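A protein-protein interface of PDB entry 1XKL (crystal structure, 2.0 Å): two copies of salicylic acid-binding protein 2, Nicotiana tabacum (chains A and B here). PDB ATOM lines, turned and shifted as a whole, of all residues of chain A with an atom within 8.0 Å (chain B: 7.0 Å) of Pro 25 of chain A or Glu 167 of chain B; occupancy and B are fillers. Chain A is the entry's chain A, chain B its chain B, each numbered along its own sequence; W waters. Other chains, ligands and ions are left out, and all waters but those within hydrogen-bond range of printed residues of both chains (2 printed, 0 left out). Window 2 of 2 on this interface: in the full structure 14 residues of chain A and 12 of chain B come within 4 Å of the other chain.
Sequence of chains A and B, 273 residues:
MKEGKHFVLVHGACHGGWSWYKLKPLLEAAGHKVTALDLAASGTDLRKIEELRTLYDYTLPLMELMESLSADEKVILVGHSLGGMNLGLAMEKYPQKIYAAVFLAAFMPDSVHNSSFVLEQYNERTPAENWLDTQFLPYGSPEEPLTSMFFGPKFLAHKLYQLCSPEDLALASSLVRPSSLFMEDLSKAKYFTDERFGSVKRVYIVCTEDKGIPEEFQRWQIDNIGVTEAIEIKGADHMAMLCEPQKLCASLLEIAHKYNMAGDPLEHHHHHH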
ATOM      1  N   LEU A   9       9.031   5.048  -8.498  1.00  0.00           N
ATOM      2  CA  LEU A   9      10.355   5.652  -8.539  1.00  0.00           C
ATOM      3  C   LEU A   9      11.243   4.997  -9.591  1.00  0.00           C
ATOM      4  O   LEU A   9      11.457   3.790  -9.586  1.00  0.00           O
ATOM      5  CB  LEU A   9      10.997   5.572  -7.150  1.00  0.00           C
ATOM      6  CG  LEU A   9      10.133   6.032  -5.964  1.00  0.00           C
ATOM      7  CD1 LEU A   9      10.986   6.029  -4.688  1.00  0.00           C
ATOM      8  CD2 LEU A   9       9.587   7.436  -6.218  1.00  0.00           C
ATOM      9  N   TRP A  18      17.616   0.369  -5.574  1.00  0.00           N
ATOM     10  CA  TRP A  18      18.310   0.573  -4.316  1.00  0.00           C
ATOM     11  C   TRP A  18      18.600   2.042  -3.998  1.00  0.00           C
ATOM     12  O   TRP A  18      18.647   2.422  -2.829  1.00  0.00           O
ATOM     13  CB  TRP A  18      19.629  -0.190  -4.312  1.00  0.00           C
ATOM     14  CG  TRP A  18      20.574   0.211  -5.402  1.00  0.00           C
ATOM     15  CD1 TRP A  18      20.720  -0.384  -6.625  1.00  0.00           C
ATOM     16  CD2 TRP A  18      21.548   1.261  -5.351  1.00  0.00           C
ATOM     17  NE1 TRP A  18      21.733   0.224  -7.334  1.00  0.00           N
ATOM     18  CE2 TRP A  18      22.257   1.236  -6.574  1.00  0.00           C
ATOM     19  CE3 TRP A  18      21.892   2.218  -4.390  1.00  0.00           C
ATOM     20  CZ2 TRP A  18      23.293   2.130  -6.860  1.00  0.00           C
ATOM     21  CZ3 TRP A  18      22.921   3.111  -4.670  1.00  0.00           C
ATOM     22  CH2 TRP A  18      23.612   3.059  -5.899  1.00  0.00           C
ATOM     23  N   TRP A  20      16.809   4.513  -4.057  1.00  0.00           N
ATOM     24  CA  TRP A  20      15.697   5.143  -3.354  1.00  0.00           C
ATOM     25  C   TRP A  20      15.499   4.607  -1.940  1.00  0.00           C
ATOM     26  O   TRP A  20      14.471   4.879  -1.316  1.00  0.00           O
ATOM     27  CB  TRP A  20      14.401   4.924  -4.133  1.00  0.00           C
ATOM     28  CG  TRP A  20      14.462   5.359  -5.564  1.00  0.00           C
ATOM     29  CD1 TRP A  20      14.636   4.561  -6.670  1.00  0.00           C
ATOM     30  CD2 TRP A  20      14.322   6.696  -6.051  1.00  0.00           C
ATOM     31  NE1 TRP A  20      14.607   5.329  -7.814  1.00  0.00           N
ATOM     32  CE2 TRP A  20      14.415   6.641  -7.461  1.00  0.00           C
ATOM     33  CE3 TRP A  20      14.127   7.937  -5.432  1.00  0.00           C
ATOM     34  CZ2 TRP A  20      14.316   7.783  -8.262  1.00  0.00           C
ATOM     35  CZ3 TRP A  20      14.030   9.076  -6.230  1.00  0.00           C
ATOM     36  CH2 TRP A  20      14.125   8.987  -7.632  1.00  0.00           C
ATOM     37  N   TYR A  21      16.472   3.869  -1.411  1.00  0.00           N
ATOM     38  CA  TYR A  21      16.285   3.279  -0.081  1.00  0.00           C
ATOM     39  C   TYR A  21      16.015   4.253   1.067  1.00  0.00           C
ATOM     40  O   TYR A  21      15.322   3.899   2.023  1.00  0.00           O
ATOM     41  CB  TYR A  21      17.458   2.349   0.270  1.00  0.00           C
ATOM     42  CG  TYR A  21      18.690   3.029   0.814  1.00  0.00           C
ATOM     43  CD1 TYR A  21      19.028   2.930   2.165  1.00  0.00           C
ATOM     44  CD2 TYR A  21      19.538   3.746  -0.025  1.00  0.00           C
ATOM     45  CE1 TYR A  21      20.184   3.527   2.670  1.00  0.00           C
ATOM     46  CE2 TYR A  21      20.693   4.349   0.468  1.00  0.00           C
ATOM     47  CZ  TYR A  21      21.010   4.232   1.816  1.00  0.00           C
ATOM     48  OH  TYR A  21      22.167   4.815   2.282  1.00  0.00           O
ATOM     49  N   LYS A  22      16.550   5.469   0.985  1.00  0.00           N
ATOM     50  CA  LYS A  22      16.317   6.464   2.037  1.00  0.00           C
ATOM     51  C   LYS A  22      14.982   7.173   1.845  1.00  0.00           C
ATOM     52  O   LYS A  22      14.332   7.564   2.816  1.00  0.00           O
ATOM     53  CB  LYS A  22      17.436   7.506   2.059  1.00  0.00           C
ATOM     54  CG  LYS A  22      18.738   7.026   2.655  1.00  0.00           C
ATOM     55  CD  LYS A  22      19.817   8.071   2.475  1.00  0.00           C
ATOM     56  CE  LYS A  22      21.027   7.771   3.337  1.00  0.00           C
ATOM     57  NZ  LYS A  22      22.154   8.692   3.022  1.00  0.00           N
ATOM     58  N   LEU A  23      14.572   7.350   0.592  1.00  0.00           N
ATOM     59  CA  LEU A  23      13.307   8.024   0.307  1.00  0.00           C
ATOM     60  C   LEU A  23      12.086   7.137   0.513  1.00  0.00           C
ATOM     61  O   LEU A  23      11.085   7.579   1.075  1.00  0.00           O
ATOM     62  CB  LEU A  23      13.283   8.555  -1.132  1.00  0.00           C
ATOM     63  CG  LEU A  23      12.020   9.347  -1.491  1.00  0.00           C
ATOM     64  CD1 LEU A  23      11.978  10.608  -0.630  1.00  0.00           C
ATOM     65  CD2 LEU A  23      12.016   9.732  -2.979  1.00  0.00           C
ATOM     66  N   LYS A  24      12.175   5.886   0.061  1.00  0.00           N
ATOM     67  CA  LYS A  24      11.057   4.944   0.152  1.00  0.00           C
ATOM     68  C   LYS A  24      10.331   4.900   1.497  1.00  0.00           C
ATOM     69  O   LYS A  24       9.112   5.027   1.540  1.00  0.00           O
ATOM     70  CB  LYS A  24      11.525   3.535  -0.238  1.00  0.00           C
ATOM     71  CG  LYS A  24      10.415   2.489  -0.318  1.00  0.00           C
ATOM     72  CD  LYS A  24      10.916   1.216  -1.031  1.00  0.00           C
ATOM     73  CE  LYS A  24       9.911   0.070  -0.949  1.00  0.00           C
ATOM     74  NZ  LYS A  24       8.588   0.419  -1.531  1.00  0.00           N
ATOM     75  N   PRO A  25      11.064   4.702   2.606  1.00  0.00           N
ATOM     76  CA  PRO A  25      10.448   4.649   3.939  1.00  0.00           C
ATOM     77  C   PRO A  25       9.670   5.929   4.255  1.00  0.00           C
ATOM     78  O   PRO A  25       8.606   5.885   4.874  1.00  0.00           O
ATOM     79  CB  PRO A  25      11.645   4.490   4.875  1.00  0.00           C
ATOM     80  CG  PRO A  25      12.672   3.834   4.026  1.00  0.00           C
ATOM     81  CD  PRO A  25      12.521   4.506   2.696  1.00  0.00           C
ATOM     82  N   LEU A  26      10.211   7.067   3.835  1.00  0.00           N
ATOM     83  CA  LEU A  26       9.566   8.359   4.085  1.00  0.00           C
ATOM     84  C   LEU A  26       8.199   8.468   3.443  1.00  0.00           C
ATOM     85  O   LEU A  26       7.252   8.942   4.064  1.00  0.00           O
ATOM     86  CB  LEU A  26      10.454   9.492   3.582  1.00  0.00           C
ATOM     87  CG  LEU A  26      11.499  10.052   4.541  1.00  0.00           C
ATOM     88  CD1 LEU A  26      11.891   9.043   5.602  1.00  0.00           C
ATOM     89  CD2 LEU A  26      12.686  10.527   3.727  1.00  0.00           C
ATOM     90  N   LEU A  27       8.105   8.044   2.189  1.00  0.00           N
ATOM     91  CA  LEU A  27       6.848   8.094   1.470  1.00  0.00           C
ATOM     92  C   LEU A  27       5.845   7.115   2.067  1.00  0.00           C
ATOM     93  O   LEU A  27       4.658   7.424   2.184  1.00  0.00           O
ATOM     94  CB  LEU A  27       7.076   7.778  -0.011  1.00  0.00           C
ATOM     95  CG  LEU A  27       7.894   8.814  -0.796  1.00  0.00           C
ATOM     96  CD1 LEU A  27       8.125   8.313  -2.215  1.00  0.00           C
ATOM     97  CD2 LEU A  27       7.150  10.147  -0.813  1.00  0.00           C
ATOM     98  N   GLU A  28       6.319   5.935   2.451  1.00  0.00           N
ATOM     99  CA  GLU A  28       5.440   4.931   3.040  1.00  0.00           C
ATOM    100  C   GLU A  28       4.981   5.403   4.413  1.00  0.00           C
ATOM    101  O   GLU A  28       3.845   5.160   4.813  1.00  0.00           O
ATOM    102  CB  GLU A  28       6.170   3.588   3.156  1.00  0.00           C
ATOM    103  CG  GLU A  28       6.759   3.110   1.833  1.00  0.00           C
ATOM    104  CD  GLU A  28       7.259   1.676   1.879  1.00  0.00           C
ATOM    105  OE1 GLU A  28       7.974   1.322   2.841  1.00  0.00           O
ATOM    106  OE2 GLU A  28       6.946   0.908   0.942  1.00  0.00           O
ATOM    107  N   ALA A  29       5.863   6.083   5.135  1.00  0.00           N
ATOM    108  CA  ALA A  29       5.501   6.592   6.450  1.00  0.00           C
ATOM    109  C   ALA A  29       4.330   7.556   6.301  1.00  0.00           C
ATOM    110  O   ALA A  29       3.496   7.678   7.197  1.00  0.00           O
ATOM    111  CB  ALA A  29       6.686   7.296   7.085  1.00  0.00           C
ATOM    112  N   ALA A  30       4.260   8.227   5.153  1.00  0.00           N
ATOM    113  CA  ALA A  30       3.187   9.185   4.888  1.00  0.00           C
ATOM    114  C   ALA A  30       1.896   8.484   4.476  1.00  0.00           C
ATOM    115  O   ALA A  30       0.895   9.137   4.172  1.00  0.00           O
ATOM    116  CB  ALA A  30       3.624  10.171   3.803  1.00  0.00           C
ATOM    117  N   GLY A  31       1.935   7.154   4.459  1.00  0.00           N
ATOM    118  CA  GLY A  31       0.765   6.371   4.102  1.00  0.00           C
ATOM    119  C   GLY A  31       0.628   6.100   2.621  1.00  0.00           C
ATOM    120  O   GLY A  31      -0.438   5.705   2.150  1.00  0.00           O
ATOM    121  N   HIS A  32       1.710   6.296   1.881  1.00  0.00           N
ATOM    122  CA  HIS A  32       1.684   6.081   0.445  1.00  0.00           C
ATOM    123  C   HIS A  32       2.369   4.780   0.053  1.00  0.00           C
ATOM    124  O   HIS A  32       3.208   4.260   0.791  1.00  0.00           O
ATOM    125  CB  HIS A  32       2.361   7.256  -0.261  1.00  0.00           C
ATOM    126  CG  HIS A  32       1.672   8.568  -0.047  1.00  0.00           C
ATOM    127  ND1 HIS A  32       0.432   8.852  -0.573  1.00  0.00           N
ATOM    128  CD2 HIS A  32       2.052   9.672   0.638  1.00  0.00           C
ATOM    129  CE1 HIS A  32       0.076  10.074  -0.222  1.00  0.00           C
ATOM    130  NE2 HIS A  32       1.041  10.593   0.514  1.00  0.00           N
ATOM    131  N   VAL A  34       4.825   2.688  -2.484  1.00  0.00           N
ATOM    132  CA  VAL A  34       6.011   3.013  -3.261  1.00  0.00           C
ATOM    133  C   VAL A  34       6.580   1.812  -4.004  1.00  0.00           C
ATOM    134  O   VAL A  34       6.653   0.709  -3.458  1.00  0.00           O
ATOM    135  CB  VAL A  34       7.122   3.578  -2.343  1.00  0.00           C
ATOM    136  CG1 VAL A  34       8.408   3.827  -3.132  1.00  0.00           C
ATOM    137  CG2 VAL A  34       6.642   4.858  -1.687  1.00  0.00           C
ATOM    138  N   MET A 241      18.060  12.152  -3.410  1.00  0.00           N
ATOM    139  CA  MET A 241      17.383  11.162  -2.568  1.00  0.00           C
ATOM    140  C   MET A 241      18.296  10.566  -1.506  1.00  0.00           C
ATOM    141  O   MET A 241      17.842   9.838  -0.618  1.00  0.00           O
ATOM    142  CB  MET A 241      16.769  10.030  -3.408  1.00  0.00           C
ATOM    143  CG  MET A 241      17.765   9.045  -3.990  1.00  0.00           C
ATOM    144  SD  MET A 241      18.685   9.757  -5.548  1.00  0.00           S
ATOM    145  CE  MET A 241      17.513   9.046  -6.902  1.00  0.00           C
ATOM    146  N   PRO A 245      16.970  13.422   1.454  1.00  0.00           N
ATOM    147  CA  PRO A 245      15.742  12.626   1.349  1.00  0.00           C
ATOM    148  C   PRO A 245      14.479  13.235   1.951  1.00  0.00           C
ATOM    149  O   PRO A 245      13.396  13.087   1.385  1.00  0.00           O
ATOM    150  CB  PRO A 245      16.125  11.308   2.020  1.00  0.00           C
ATOM    151  CG  PRO A 245      17.143  11.724   3.023  1.00  0.00           C
ATOM    152  CD  PRO A 245      17.990  12.692   2.228  1.00  0.00           C
ATOM    153  N   GLN A 246      14.606  13.906   3.093  1.00  0.00           N
ATOM    154  CA  GLN A 246      13.437  14.505   3.720  1.00  0.00           C
ATOM    155  C   GLN A 246      12.951  15.717   2.919  1.00  0.00           C
ATOM    156  O   GLN A 246      11.746  15.930   2.791  1.00  0.00           O
ATOM    157  CB  GLN A 246      13.745  14.885   5.178  1.00  0.00           C
ATOM    158  CG  GLN A 246      14.388  13.745   5.973  1.00  0.00           C
ATOM    159  CD  GLN A 246      14.701  14.106   7.415  1.00  0.00           C
ATOM    160  OE1 GLN A 246      13.829  14.050   8.284  1.00  0.00           O
ATOM    161  NE2 GLN A 246      15.950  14.487   7.672  1.00  0.00           N
ATOM    162  N   CYS A 249      11.214  14.267  -0.076  1.00  0.00           N
ATOM    163  CA  CYS A 249       9.942  13.659   0.300  1.00  0.00           C
ATOM    164  C   CYS A 249       8.863  14.729   0.473  1.00  0.00           C
ATOM    165  O   CYS A 249       7.737  14.566  -0.001  1.00  0.00           O
ATOM    166  CB  CYS A 249      10.091  12.857   1.603  1.00  0.00           C
ATOM    167  SG  CYS A 249       8.541  12.127   2.231  1.00  0.00           S
ATOM    168  N   TYR B  21      28.589  -1.252   3.393  1.00  0.00           N
ATOM    169  CA  TYR B  21      28.686   0.164   3.071  1.00  0.00           C
ATOM    170  C   TYR B  21      28.859   1.124   4.254  1.00  0.00           C
ATOM    171  O   TYR B  21      29.387   2.222   4.079  1.00  0.00           O
ATOM    172  CB  TYR B  21      27.494   0.564   2.193  1.00  0.00           C
ATOM    173  CG  TYR B  21      26.232   0.956   2.914  1.00  0.00           C
ATOM    174  CD1 TYR B  21      25.948   2.299   3.171  1.00  0.00           C
ATOM    175  CD2 TYR B  21      25.303  -0.004   3.313  1.00  0.00           C
ATOM    176  CE1 TYR B  21      24.773   2.680   3.802  1.00  0.00           C
ATOM    177  CE2 TYR B  21      24.120   0.365   3.947  1.00  0.00           C
ATOM    178  CZ  TYR B  21      23.861   1.710   4.186  1.00  0.00           C
ATOM    179  OH  TYR B  21      22.680   2.085   4.781  1.00  0.00           O
ATOM    180  N   LYS B  22      28.439   0.721   5.453  1.00  0.00           N
ATOM    181  CA  LYS B  22      28.597   1.584   6.624  1.00  0.00           C
ATOM    182  C   LYS B  22      29.922   1.326   7.330  1.00  0.00           C
ATOM    183  O   LYS B  22      30.520   2.230   7.926  1.00  0.00           O
ATOM    184  CB  LYS B  22      27.458   1.374   7.620  1.00  0.00           C
ATOM    185  CG  LYS B  22      26.120   1.894   7.150  1.00  0.00           C
ATOM    186  CD  LYS B  22      25.069   1.733   8.233  1.00  0.00           C
ATOM    187  CE  LYS B  22      23.737   2.307   7.801  1.00  0.00           C
ATOM    188  NZ  LYS B  22      22.719   2.168   8.884  1.00  0.00           N
ATOM    189  N   CYS B 164      17.297  -2.966  12.947  1.00  0.00           N
ATOM    190  CA  CYS B 164      17.892  -2.044  11.976  1.00  0.00           C
ATOM    191  C   CYS B 164      16.918  -0.949  11.539  1.00  0.00           C
ATOM    192  O   CYS B 164      15.711  -1.076  11.707  1.00  0.00           O
ATOM    193  CB  CYS B 164      18.362  -2.811  10.735  1.00  0.00           C
ATOM    194  SG  CYS B 164      19.847  -3.793  10.984  1.00  0.00           S
ATOM    195  N   SER B 165      17.460   0.121  10.962  1.00  0.00           N
ATOM    196  CA  SER B 165      16.649   1.242  10.491  1.00  0.00           C
ATOM    197  C   SER B 165      15.756   0.841   9.322  1.00  0.00           C
ATOM    198  O   SER B 165      16.033  -0.132   8.613  1.00  0.00           O
ATOM    199  CB  SER B 165      17.545   2.410  10.079  1.00  0.00           C
ATOM    200  OG  SER B 165      18.443   2.045   9.036  1.00  0.00           O
ATOM    201  N   PRO B 166      14.661   1.585   9.107  1.00  0.00           N
ATOM    202  CA  PRO B 166      13.735   1.287   8.008  1.00  0.00           C
ATOM    203  C   PRO B 166      14.408   1.471   6.645  1.00  0.00           C
ATOM    204  O   PRO B 166      14.011   0.852   5.665  1.00  0.00           O
ATOM    205  CB  PRO B 166      12.601   2.283   8.237  1.00  0.00           C
ATOM    206  CG  PRO B 166      13.323   3.460   8.829  1.00  0.00           C
ATOM    207  CD  PRO B 166      14.229   2.789   9.837  1.00  0.00           C
ATOM    208  N   GLU B 167      15.431   2.318   6.599  1.00  0.00           N
ATOM    209  CA  GLU B 167      16.150   2.554   5.363  1.00  0.00           C
ATOM    210  C   GLU B 167      16.941   1.299   5.020  1.00  0.00           C
ATOM    211  O   GLU B 167      16.945   0.849   3.874  1.00  0.00           O
ATOM    212  CB  GLU B 167      17.095   3.748   5.507  1.00  0.00           C
ATOM    213  CG  GLU B 167      16.408   5.119   5.621  1.00  0.00           C
ATOM    214  CD  GLU B 167      15.686   5.331   6.945  1.00  0.00           C
ATOM    215  OE1 GLU B 167      16.191   4.844   7.979  1.00  0.00           O
ATOM    216  OE2 GLU B 167      14.622   6.001   6.954  1.00  0.00           O
ATOM    217  N   ASP B 168      17.606   0.730   6.019  1.00  0.00           N
ATOM    218  CA  ASP B 168      18.385  -0.479   5.798  1.00  0.00           C
ATOM    219  C   ASP B 168      17.504  -1.639   5.342  1.00  0.00           C
ATOM    220  O   ASP B 168      17.906  -2.409   4.480  1.00  0.00           O
ATOM    221  CB  ASP B 168      19.172  -0.828   7.064  1.00  0.00           C
ATOM    222  CG  ASP B 168      20.387   0.060   7.236  1.00  0.00           C
ATOM    223  OD1 ASP B 168      20.830   0.280   8.378  1.00  0.00           O
ATOM    224  OD2 ASP B 168      20.914   0.545   6.208  1.00  0.00           O
ATOM    225  N   LEU B 169      16.294  -1.748   5.884  1.00  0.00           N
ATOM    226  CA  LEU B 169      15.396  -2.826   5.482  1.00  0.00           C
ATOM    227  C   LEU B 169      14.964  -2.653   4.028  1.00  0.00           C
ATOM    228  O   LEU B 169      14.808  -3.631   3.288  1.00  0.00           O
ATOM    229  CB  LEU B 169      14.158  -2.856   6.375  1.00  0.00           C
ATOM    230  CG  LEU B 169      13.091  -3.880   5.979  1.00  0.00           C
ATOM    231  CD1 LEU B 169      13.696  -5.283   5.950  1.00  0.00           C
ATOM    232  CD2 LEU B 169      11.936  -3.822   6.970  1.00  0.00           C
ATOM    233  N   ALA B 170      14.755  -1.400   3.636  1.00  0.00           N
ATOM    234  CA  ALA B 170      14.350  -1.065   2.271  1.00  0.00           C
ATOM    235  C   ALA B 170      15.513  -1.373   1.331  1.00  0.00           C
ATOM    236  O   ALA B 170      15.317  -1.868   0.223  1.00  0.00           O
ATOM    237  CB  ALA B 170      13.982   0.411   2.185  1.00  0.00           C
ATOM    238  N   LEU B 171      16.726  -1.076   1.776  1.00  0.00           N
ATOM    239  CA  LEU B 171      17.898  -1.348   0.963  1.00  0.00           C
ATOM    240  C   LEU B 171      17.999  -2.855   0.733  1.00  0.00           C
ATOM    241  O   LEU B 171      18.178  -3.310  -0.393  1.00  0.00           O
ATOM    242  CB  LEU B 171      19.157  -0.839   1.657  1.00  0.00           C
ATOM    243  CG  LEU B 171      20.474  -0.971   0.887  1.00  0.00           C
ATOM    244  CD1 LEU B 171      20.422  -0.183  -0.412  1.00  0.00           C
ATOM    245  CD2 LEU B 171      21.613  -0.470   1.768  1.00  0.00           C
ATOM    246  N   ALA B 172      17.866  -3.635   1.799  1.00  0.00           N
ATOM    247  CA  ALA B 172      17.953  -5.081   1.663  1.00  0.00           C
ATOM    248  C   ALA B 172      16.874  -5.647   0.748  1.00  0.00           C
ATOM    249  O   ALA B 172      17.158  -6.482  -0.116  1.00  0.00           O
ATOM    250  CB  ALA B 172      17.884  -5.744   3.030  1.00  0.00           C
ATOM    251  N   SER B 173      15.634  -5.201   0.929  1.00  0.00           N
ATOM    252  CA  SER B 173      14.530  -5.696   0.107  1.00  0.00           C
ATOM    253  C   SER B 173      14.722  -5.454  -1.390  1.00  0.00           C
ATOM    254  O   SER B 173      14.196  -6.197  -2.217  1.00  0.00           O
ATOM    255  CB  SER B 173      13.212  -5.068   0.563  1.00  0.00           C
ATOM    256  OG  SER B 173      12.920  -5.447   1.896  1.00  0.00           O
HETATM  257  O   HOH W   1      22.261   4.830   5.086  1.00  0.00           O
HETATM  258  O   HOH W   2      15.355   8.258   5.261  1.00  0.00           O
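Leu 171 of chain B touches Trp 18 of chain A (CD1 to O, 3.97 Å).
Tyr 21 of chain A touches Tyr 21 of chain B.
Glu 167 of chain B touches Tyr 21 of chain A.
O of Tyr 21 of chain A touches CB of Ala 170 of chain B (3.7 Å).
Tyr 21 of chain A touches Leu 171 of chain B (CB to CA, 3.8 Å).
CG of Glu 167 of chain B touches CA of Lys 22 of chain A (3.8 Å).
CG of Pro 25 of chain A touches O of Pro 166 of chain B, at 3.7 Å.
Glu 167 of chain B touches Pro 25 of chain A (OE2 to CB, 3.9 Å).
Water W2 bridges the backbone carbonyl oxygen (O) of Lys 22 of chain A (2.7 Å) and the side-chain carboxylate (OE2) of Glu 167 of chain B (2.9 Å).
Water W1 lies within hydrogen-bond range of OH of Tyr 21 of chain B (2.8 Å) and OH of Tyr 21 of chain A (2.8 Å).
Printed residues of chain A that touch a printed residue of chain B: Trp 18, Tyr 21, Lys 22 and Pro 25.
Hydrophobic or aromatic side chains of chain A that line the printed part of chain B: Trp 18, Tyr 21 and Pro 25.
Along chain A the printed residues that touch a printed residue of chain B span positions 18 to 25.
Of the 12 printed residues of chain B, 5 touch a printed residue of chain A.
Printed residues of chain B that touch a printed residue of chain A: Tyr 21, Pro 166, Glu 167, Ala 170 and Leu 171.
Among the printed residues, no Asp or Glu carboxylate lies within 4 Å of a Lys or Arg side-chain nitrogen of the other chain.
The side-chain hydroxyl (OH) of Tyr 21 of chain B sits at hydrogen-bond distance from the side-chain carboxylate (OD2) of Asp 168 of chain B, 2.7 Å away.
Tyr 21 of chain B touches its own counterpart, Tyr 21 of chain A.
2 positions are printed for both chains.
Of the printed residues of chain B, Trp 18 of chain A touches Leu 171 (3.97 Å).
Pro 25 of chain A touches two residues of chain B.
Pro 166 of chain B touches just one residue of chain A: Pro 25.
Glu 167 of chain B touches just these residues of chain A: Tyr 21 (3.4 Å), Lys 22 (3.8 Å) and Pro 25 (3.9 Å).
Of the printed residues of chain A, Leu 171 of chain B touches Trp 18 and Tyr 21.
The nearest residue of chain B that does not touch Pro 25 of chain A is Ala 170 of chain B (4.1 Å).
The nearest printed residue of chain A that does not touch Ala 170 of chain B is Pro 25 of chain A (4.1 Å).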
